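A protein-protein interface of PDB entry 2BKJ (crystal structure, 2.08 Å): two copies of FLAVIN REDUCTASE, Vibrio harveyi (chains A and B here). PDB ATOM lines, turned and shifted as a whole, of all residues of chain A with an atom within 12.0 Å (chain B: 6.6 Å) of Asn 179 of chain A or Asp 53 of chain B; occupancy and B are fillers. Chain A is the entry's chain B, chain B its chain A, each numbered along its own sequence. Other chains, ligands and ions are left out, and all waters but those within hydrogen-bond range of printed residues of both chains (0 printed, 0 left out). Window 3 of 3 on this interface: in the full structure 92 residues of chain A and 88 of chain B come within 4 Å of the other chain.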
ATOM      1  N   ALA A 172       2.928 -16.614  -3.320  1.00  0.00           N
ATOM      2  CA  ALA A 172       3.540 -15.294  -3.255  1.00  0.00           C
ATOM      3  C   ALA A 172       3.173 -14.372  -4.416  1.00  0.00           C
ATOM      4  O   ALA A 172       3.019 -13.167  -4.217  1.00  0.00           O
ATOM      5  CB  ALA A 172       5.053 -15.423  -3.144  1.00  0.00           C
ATOM      6  N   HIS A 173       3.015 -14.930  -5.616  1.00  0.00           N
ATOM      7  CA  HIS A 173       2.677 -14.113  -6.781  1.00  0.00           C
ATOM      8  C   HIS A 173       1.265 -13.522  -6.736  1.00  0.00           C
ATOM      9  O   HIS A 173       0.940 -12.612  -7.501  1.00  0.00           O
ATOM     10  CB  HIS A 173       2.926 -14.877  -8.093  1.00  0.00           C
ATOM     11  CG  HIS A 173       1.963 -15.995  -8.353  1.00  0.00           C
ATOM     12  ND1 HIS A 173       2.234 -17.305  -8.027  1.00  0.00           N
ATOM     13  CD2 HIS A 173       0.745 -16.001  -8.951  1.00  0.00           C
ATOM     14  CE1 HIS A 173       1.230 -18.071  -8.412  1.00  0.00           C
ATOM     15  NE2 HIS A 173       0.313 -17.304  -8.976  1.00  0.00           N
ATOM     16  N   VAL A 174       0.432 -14.038  -5.837  1.00  0.00           N
ATOM     17  CA  VAL A 174      -0.931 -13.538  -5.680  1.00  0.00           C
ATOM     18  C   VAL A 174      -0.948 -12.449  -4.605  1.00  0.00           C
ATOM     19  O   VAL A 174      -1.597 -11.415  -4.763  1.00  0.00           O
ATOM     20  CB  VAL A 174      -1.912 -14.673  -5.274  1.00  0.00           C
ATOM     21  CG1 VAL A 174      -3.294 -14.107  -4.979  1.00  0.00           C
ATOM     22  CG2 VAL A 174      -2.009 -15.709  -6.383  1.00  0.00           C
ATOM     23  N   VAL A 175      -0.201 -12.681  -3.528  1.00  0.00           N
ATOM     24  CA  VAL A 175      -0.128 -11.750  -2.407  1.00  0.00           C
ATOM     25  C   VAL A 175       0.804 -10.563  -2.645  1.00  0.00           C
ATOM     26  O   VAL A 175       0.539  -9.458  -2.168  1.00  0.00           O
ATOM     27  CB  VAL A 175       0.288 -12.489  -1.107  1.00  0.00           C
ATOM     28  CG1 VAL A 175       0.477 -11.503   0.044  1.00  0.00           C
ATOM     29  CG2 VAL A 175      -0.768 -13.524  -0.743  1.00  0.00           C
ATOM     30  N   VAL A 176       1.894 -10.795  -3.371  1.00  0.00           N
ATOM     31  CA  VAL A 176       2.860  -9.738  -3.658  1.00  0.00           C
ATOM     32  C   VAL A 176       2.641  -9.118  -5.037  1.00  0.00           C
ATOM     33  O   VAL A 176       2.551  -9.822  -6.047  1.00  0.00           O
ATOM     34  CB  VAL A 176       4.312 -10.257  -3.537  1.00  0.00           C
ATOM     35  CG1 VAL A 176       5.304  -9.119  -3.730  1.00  0.00           C
ATOM     36  CG2 VAL A 176       4.521 -10.915  -2.180  1.00  0.00           C
ATOM     37  N   HIS A 177       2.544  -7.792  -5.060  1.00  0.00           N
ATOM     38  CA  HIS A 177       2.332  -7.026  -6.285  1.00  0.00           C
ATOM     39  C   HIS A 177       3.578  -6.217  -6.607  1.00  0.00           C
ATOM     40  O   HIS A 177       4.202  -5.647  -5.711  1.00  0.00           O
ATOM     41  CB  HIS A 177       1.152  -6.067  -6.110  1.00  0.00           C
ATOM     42  CG  HIS A 177      -0.122  -6.744  -5.720  1.00  0.00           C
ATOM     43  ND1 HIS A 177      -1.169  -6.920  -6.595  1.00  0.00           N
ATOM     44  CD2 HIS A 177      -0.511  -7.302  -4.548  1.00  0.00           C
ATOM     45  CE1 HIS A 177      -2.149  -7.560  -5.983  1.00  0.00           C
ATOM     46  NE2 HIS A 177      -1.776  -7.803  -4.740  1.00  0.00           N
ATOM     47  N   GLU A 178       3.933  -6.158  -7.885  1.00  0.00           N
ATOM     48  CA  GLU A 178       5.106  -5.404  -8.308  1.00  0.00           C
ATOM     49  C   GLU A 178       4.739  -3.999  -8.785  1.00  0.00           C
ATOM     50  O   GLU A 178       4.085  -3.839  -9.817  1.00  0.00           O
ATOM     51  CB  GLU A 178       5.853  -6.155  -9.415  1.00  0.00           C
ATOM     52  N   ASN A 179       5.127  -3.000  -7.991  1.00  0.00           N
ATOM     53  CA  ASN A 179       4.907  -1.577  -8.285  1.00  0.00           C
ATOM     54  C   ASN A 179       3.477  -1.059  -8.300  1.00  0.00           C
ATOM     55  O   ASN A 179       3.228   0.096  -7.945  1.00  0.00           O
ATOM     56  CB  ASN A 179       5.606  -1.193  -9.591  1.00  0.00           C
ATOM     57  CG  ASN A 179       7.106  -1.334  -9.500  1.00  0.00           C
ATOM     58  OD1 ASN A 179       7.731  -0.808  -8.579  1.00  0.00           O
ATOM     59  ND2 ASN A 179       7.694  -2.056 -10.444  1.00  0.00           N
ATOM     60  N   GLN A 180       2.543  -1.900  -8.726  1.00  0.00           N
ATOM     61  CA  GLN A 180       1.140  -1.515  -8.794  1.00  0.00           C
ATOM     62  C   GLN A 180       0.275  -2.728  -8.507  1.00  0.00           C
ATOM     63  O   GLN A 180       0.706  -3.864  -8.696  1.00  0.00           O
ATOM     64  CB  GLN A 180       0.808  -0.959 -10.187  1.00  0.00           C
ATOM     65  N   TYR A 181      -0.945  -2.479  -8.046  1.00  0.00           N
ATOM     66  CA  TYR A 181      -1.879  -3.551  -7.733  1.00  0.00           C
ATOM     67  C   TYR A 181      -2.269  -4.294  -9.007  1.00  0.00           C
ATOM     68  O   TYR A 181      -2.683  -3.682  -9.993  1.00  0.00           O
ATOM     69  CB  TYR A 181      -3.124  -2.984  -7.052  1.00  0.00           C
ATOM     70  CG  TYR A 181      -4.014  -4.034  -6.423  1.00  0.00           C
ATOM     71  CD1 TYR A 181      -5.021  -4.655  -7.161  1.00  0.00           C
ATOM     72  CD2 TYR A 181      -3.856  -4.399  -5.085  1.00  0.00           C
ATOM     73  CE1 TYR A 181      -5.854  -5.612  -6.580  1.00  0.00           C
ATOM     74  CE2 TYR A 181      -4.681  -5.352  -4.495  1.00  0.00           C
ATOM     75  CZ  TYR A 181      -5.676  -5.954  -5.248  1.00  0.00           C
ATOM     76  OH  TYR A 181      -6.498  -6.894  -4.672  1.00  0.00           O
ATOM     77  N   GLN A 182      -2.120  -5.614  -8.981  1.00  0.00           N
ATOM     78  CA  GLN A 182      -2.445  -6.451 -10.131  1.00  0.00           C
ATOM     79  C   GLN A 182      -3.800  -7.129  -9.964  1.00  0.00           C
ATOM     80  O   GLN A 182      -4.200  -7.466  -8.849  1.00  0.00           O
ATOM     81  CB  GLN A 182      -1.351  -7.504 -10.340  1.00  0.00           C
ATOM     82  N   GLU A 183      -4.503  -7.321 -11.077  1.00  0.00           N
ATOM     83  CA  GLU A 183      -5.814  -7.960 -11.064  1.00  0.00           C
ATOM     84  C   GLU A 183      -5.689  -9.440 -10.711  1.00  0.00           C
ATOM     85  O   GLU A 183      -4.723 -10.101 -11.095  1.00  0.00           O
ATOM     86  CB  GLU A 183      -6.502  -7.800 -12.424  1.00  0.00           C
ATOM     87  N   VAL B  49       2.870  -4.627  -1.718  1.00  0.00           N
ATOM     88  CA  VAL B  49       3.265  -4.010  -2.976  1.00  0.00           C
ATOM     89  C   VAL B  49       4.762  -3.729  -2.916  1.00  0.00           C
ATOM     90  O   VAL B  49       5.216  -2.905  -2.123  1.00  0.00           O
ATOM     91  CB  VAL B  49       2.503  -2.692  -3.259  1.00  0.00           C
ATOM     92  CG1 VAL B  49       2.948  -2.111  -4.596  1.00  0.00           C
ATOM     93  CG2 VAL B  49       1.000  -2.939  -3.275  1.00  0.00           C
ATOM     94  N   ARG B  50       5.527  -4.472  -3.712  1.00  0.00           N
ATOM     95  CA  ARG B  50       6.975  -4.305  -3.784  1.00  0.00           C
ATOM     96  C   ARG B  50       7.272  -3.219  -4.819  1.00  0.00           C
ATOM     97  O   ARG B  50       6.943  -3.370  -5.997  1.00  0.00           O
ATOM     98  CB  ARG B  50       7.637  -5.619  -4.206  1.00  0.00           C
ATOM     99  CG  ARG B  50       9.147  -5.532  -4.312  1.00  0.00           C
ATOM    100  CD  ARG B  50       9.721  -6.735  -5.026  1.00  0.00           C
ATOM    101  NE  ARG B  50      11.166  -6.618  -5.189  1.00  0.00           N
ATOM    102  CZ  ARG B  50      11.849  -7.114  -6.216  1.00  0.00           C
ATOM    103  NH1 ARG B  50      11.221  -7.765  -7.187  1.00  0.00           N
ATOM    104  NH2 ARG B  50      13.166  -6.971  -6.263  1.00  0.00           N
ATOM    105  N   VAL B  51       7.899  -2.131  -4.380  1.00  0.00           N
ATOM    106  CA  VAL B  51       8.207  -1.016  -5.272  1.00  0.00           C
ATOM    107  C   VAL B  51       9.655  -1.005  -5.758  1.00  0.00           C
ATOM    108  O   VAL B  51      10.568  -0.632  -5.022  1.00  0.00           O
ATOM    109  CB  VAL B  51       7.876   0.340  -4.599  1.00  0.00           C
ATOM    110  CG1 VAL B  51       8.045   1.483  -5.590  1.00  0.00           C
ATOM    111  CG2 VAL B  51       6.452   0.319  -4.044  1.00  0.00           C
ATOM    112  N   THR B  52       9.852  -1.413  -7.009  1.00  0.00           N
ATOM    113  CA  THR B  52      11.178  -1.449  -7.618  1.00  0.00           C
ATOM    114  C   THR B  52      11.427  -0.264  -8.553  1.00  0.00           C
ATOM    115  O   THR B  52      12.574   0.061  -8.863  1.00  0.00           O
ATOM    116  CB  THR B  52      11.403  -2.759  -8.399  1.00  0.00           C
ATOM    117  OG1 THR B  52      10.331  -2.957  -9.331  1.00  0.00           O
ATOM    118  CG2 THR B  52      11.468  -3.934  -7.451  1.00  0.00           C
ATOM    119  N   ASP B  53      10.350   0.367  -9.010  1.00  0.00           N
ATOM    120  CA  ASP B  53      10.441   1.521  -9.901  1.00  0.00           C
ATOM    121  C   ASP B  53      11.061   2.701  -9.148  1.00  0.00           C
ATOM    122  O   ASP B  53      10.500   3.176  -8.158  1.00  0.00           O
ATOM    123  CB  ASP B  53       9.047   1.889 -10.417  1.00  0.00           C
ATOM    124  CG  ASP B  53       9.079   3.002 -11.442  1.00  0.00           C
ATOM    125  OD1 ASP B  53       9.265   2.703 -12.639  1.00  0.00           O
ATOM    126  OD2 ASP B  53       8.920   4.175 -11.054  1.00  0.00           O
ATOM    127  N   SER B  54      12.209   3.177  -9.630  1.00  0.00           N
ATOM    128  CA  SER B  54      12.928   4.283  -8.993  1.00  0.00           C
ATOM    129  C   SER B  54      12.165   5.607  -8.894  1.00  0.00           C
ATOM    130  O   SER B  54      12.380   6.375  -7.960  1.00  0.00           O
ATOM    131  CB  SER B  54      14.287   4.503  -9.669  1.00  0.00           C
ATOM    132  OG  SER B  54      14.133   4.902 -11.019  1.00  0.00           O
ATOM    133  N   GLU B  55      11.290   5.883  -9.855  1.00  0.00           N
ATOM    134  CA  GLU B  55      10.516   7.120  -9.816  1.00  0.00           C
ATOM    135  C   GLU B  55       9.416   7.051  -8.765  1.00  0.00           C
ATOM    136  O   GLU B  55       9.140   8.043  -8.089  1.00  0.00           O
ATOM    137  CB  GLU B  55       9.937   7.452 -11.191  1.00  0.00           C
ATOM    138  CG  GLU B  55      11.000   7.794 -12.217  1.00  0.00           C
ATOM    139  CD  GLU B  55      11.956   8.878 -11.736  1.00  0.00           C
ATOM    140  OE1 GLU B  55      11.479   9.956 -11.311  1.00  0.00           O
ATOM    141  OE2 GLU B  55      13.186   8.647 -11.782  1.00  0.00           O
ATOM    142  N   LYS B  56       8.792   5.884  -8.630  1.00  0.00           N
ATOM    143  CA  LYS B  56       7.746   5.702  -7.630  1.00  0.00           C
ATOM    144  C   LYS B  56       8.373   5.753  -6.241  1.00  0.00           C
ATOM    145  O   LYS B  56       7.768   6.265  -5.305  1.00  0.00           O
ATOM    146  CB  LYS B  56       6.997   4.383  -7.835  1.00  0.00           C
ATOM    147  CG  LYS B  56       6.039   4.403  -9.013  1.00  0.00           C
ATOM    148  CD  LYS B  56       5.051   3.256  -8.949  1.00  0.00           C
ATOM    149  CE  LYS B  56       4.026   3.366 -10.066  1.00  0.00           C
ATOM    150  NZ  LYS B  56       2.939   2.365  -9.917  1.00  0.00           N
ATOM    151  N   ARG B  57       9.595   5.236  -6.126  1.00  0.00           N
ATOM    152  CA  ARG B  57      10.333   5.248  -4.863  1.00  0.00           C
ATOM    153  C   ARG B  57      10.545   6.685  -4.413  1.00  0.00           C
ATOM    154  O   ARG B  57      10.350   7.012  -3.242  1.00  0.00           O
ATOM    155  CB  ARG B  57      11.701   4.592  -5.035  1.00  0.00           C
ATOM    156  CG  ARG B  57      11.696   3.085  -5.027  1.00  0.00           C
ATOM    157  CD  ARG B  57      11.608   2.524  -3.619  1.00  0.00           C
ATOM    158  NE  ARG B  57      12.179   1.183  -3.598  1.00  0.00           N
ATOM    159  CZ  ARG B  57      13.333   0.867  -3.020  1.00  0.00           C
ATOM    160  NH1 ARG B  57      14.040   1.794  -2.388  1.00  0.00           N
ATOM    161  NH2 ARG B  57      13.820  -0.360  -3.142  1.00  0.00           N
ATOM    162  N   ASN B  58      10.952   7.533  -5.355  1.00  0.00           N
ATOM    163  CA  ASN B  58      11.192   8.944  -5.079  1.00  0.00           C
ATOM    164  C   ASN B  58       9.914   9.615  -4.592  1.00  0.00           C
ATOM    165  O   ASN B  58       9.933  10.358  -3.612  1.00  0.00           O
ATOM    166  CB  ASN B  58      11.718   9.653  -6.332  1.00  0.00           C
ATOM    167  N   GLU B  59       8.802   9.326  -5.263  1.00  0.00           N
ATOM    168  CA  GLU B  59       7.509   9.894  -4.895  1.00  0.00           C
ATOM    169  C   GLU B  59       7.052   9.403  -3.522  1.00  0.00           C
ATOM    170  O   GLU B  59       6.470  10.164  -2.750  1.00  0.00           O
ATOM    171  CB  GLU B  59       6.454   9.554  -5.945  1.00  0.00           C
ATOM    172  CG  GLU B  59       6.704  10.177  -7.306  1.00  0.00           C
ATOM    173  CD  GLU B  59       5.610   9.841  -8.300  1.00  0.00           C
ATOM    174  OE1 GLU B  59       4.534  10.476  -8.240  1.00  0.00           O
ATOM    175  OE2 GLU B  59       5.817   8.932  -9.135  1.00  0.00           O
ATOM    176  N   LEU B 142      -1.174   6.239  -6.350  1.00  0.00           N
ATOM    177  CA  LEU B 142       0.119   5.915  -6.960  1.00  0.00           C
ATOM    178  C   LEU B 142       0.305   4.411  -7.157  1.00  0.00           C
ATOM    179  O   LEU B 142       0.832   3.970  -8.179  1.00  0.00           O
ATOM    180  CB  LEU B 142       1.270   6.477  -6.114  1.00  0.00           C
ATOM    181  CG  LEU B 142       2.696   6.256  -6.639  1.00  0.00           C
ATOM    182  CD1 LEU B 142       2.872   6.928  -7.996  1.00  0.00           C
ATOM    183  CD2 LEU B 142       3.709   6.799  -5.648  1.00  0.00           C
ATOM    184  N   LEU B 143      -0.141   3.632  -6.175  1.00  0.00           N
ATOM    185  CA  LEU B 143      -0.028   2.179  -6.229  1.00  0.00           C
ATOM    186  C   LEU B 143      -1.237   1.527  -6.895  1.00  0.00           C
ATOM    187  O   LEU B 143      -1.292   0.305  -7.030  1.00  0.00           O
ATOM    188  CB  LEU B 143       0.169   1.616  -4.822  1.00  0.00           C
ATOM    189  CG  LEU B 143       1.380   2.160  -4.057  1.00  0.00           C
ATOM    190  CD1 LEU B 143       1.440   1.526  -2.677  1.00  0.00           C
ATOM    191  CD2 LEU B 143       2.668   1.892  -4.834  1.00  0.00           C
ATOM    192  N   GLY B 144      -2.207   2.349  -7.292  1.00  0.00           N
ATOM    193  CA  GLY B 144      -3.405   1.851  -7.952  1.00  0.00           C
ATOM    194  C   GLY B 144      -4.264   0.903  -7.135  1.00  0.00           C
ATOM    195  O   GLY B 144      -4.801  -0.066  -7.676  1.00  0.00           O
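CA of Val 49 of chain B touches O of His 177 of chain A, at 3.3 Å. Arg 50 of chain B touches Glu 178 of chain A. Asn 179 of chain A touches Val 49 of chain B (C to CG1, 3.9 Å). Val 51 of chain B touches Asn 179 of chain A. CD2 of Leu 143 of chain B touches O of Asn 179 of chain A (3.6 Å). Gln 180 of chain A touches Lys 56 of chain B (CB to NZ, 3.96 Å). O of Leu 143 of chain B touches CA of Gln 180 of chain A (3.5 Å). Gly 144 of chain B touches Tyr 181 of chain A (O to CB, 3.4 Å).
Of the 14 printed residues of chain B, 8 touch a printed residue of chain A. Hydrophobic or aromatic side chains of chain B within 4 Å of the printed part of chain A: Val 49, Val 51 and Leu 143. Among the printed residues, 14 pairs touch across the chains. Among the printed residues, no Asp or Glu carboxylate lies within 4 Å of a Lys or Arg side-chain nitrogen of the other chain.
No position is printed for both chains. Of the 14 pairs that touch across the chains among the printed residues, none has its exchanged pair printed and touching as well.
O of Leu 143 of chain B lies within hydrogen-bond range of N of Tyr 181 of chain A. The backbone NH (N) of Asn 179 of chain A sits at hydrogen-bond distance from the backbone carbonyl oxygen (O) of Arg 50 of chain B (2.7 Å). OD1 of Asn 179 of chain A lies within hydrogen-bond range of N of Asp 53 of chain B. The backbone NH (N) of Thr 52 of chain B is in hydrogen-bond range of the side-chain amide oxygen (OD1) of Asn 179 of chain A (2.7 Å). O of His 177 of chain A sits at hydrogen-bond distance from N of Arg 50 of chain B, at 2.7 Å. The side-chain amino group (NZ) of Lys 56 of chain B is in hydrogen-bond range of the backbone carbonyl oxygen (O) of Asn 179 of chain A (3.0 Å).
N of Lys 56 of chain B sits at hydrogen-bond distance from OD2 of Asp 53 of chain B (3.0 Å). NZ of Lys 56 of chain B lies within hydrogen-bond range of O of Leu 142 of chain B. ND1 of His 177 of chain A sits at hydrogen-bond distance from N of Gln 182 of chain A. The backbone NH (N) of Glu 55 of chain B is in hydrogen-bond range of the side-chain carboxylate (OD2) of Asp 53 of chain B, at 3.2 Å. The backbone carbonyl oxygen (O) of Val 51 of chain B is in hydrogen-bond range of the guanidinium group (NE) of Arg 57 of chain B (2.8 Å).
Of chain B, only Val 49 (3.9 Å), Arg 50 (2.7 Å), Val 51 (3.3 Å), Thr 52 (2.7 Å), Asp 53 (2.9 Å), Lys 56 (3.0 Å) and Leu 143 (3.6 Å) come within 4 Å of Asn 179 of chain A. Asp 53 of chain B touches just one residue of chain A: Asn 179 (2.9 Å). Of chain A, only His 177 (3.3 Å) and Asn 179 (3.9 Å) come within 4 Å of Val 49 of chain B. Val 51 of chain B touches just one residue of chain A: Asn 179. Thr 52 of chain B touches just one residue of chain A: Asn 179. No residue of chain A comes within 4 Å of Ser 54 of chain B. No residue of chain A comes within 4 Å of Glu 55 of chain B. Of chain A, only Asn 179 and Gln 180 come within 4 Å of Lys 56 of chain B. Of chain A, only Asn 179 (3.6 Å), Gln 180 (3.5 Å) and Tyr 181 (3.0 Å) come within 4 Å of Leu 143 of chain B. Printed residues of chain A within 4 Å of Arg 50 of chain B: His 177, Glu 178 and Asn 179. Printed residues of chain B within 4 Å of His 177 of chain A: Val 49 (3.3 Å) and Arg 50 (2.7 Å). His 173 of chain A touches none of the printed residues of chain B. Asn 58 of chain B touches none of the printed residues of chain A.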
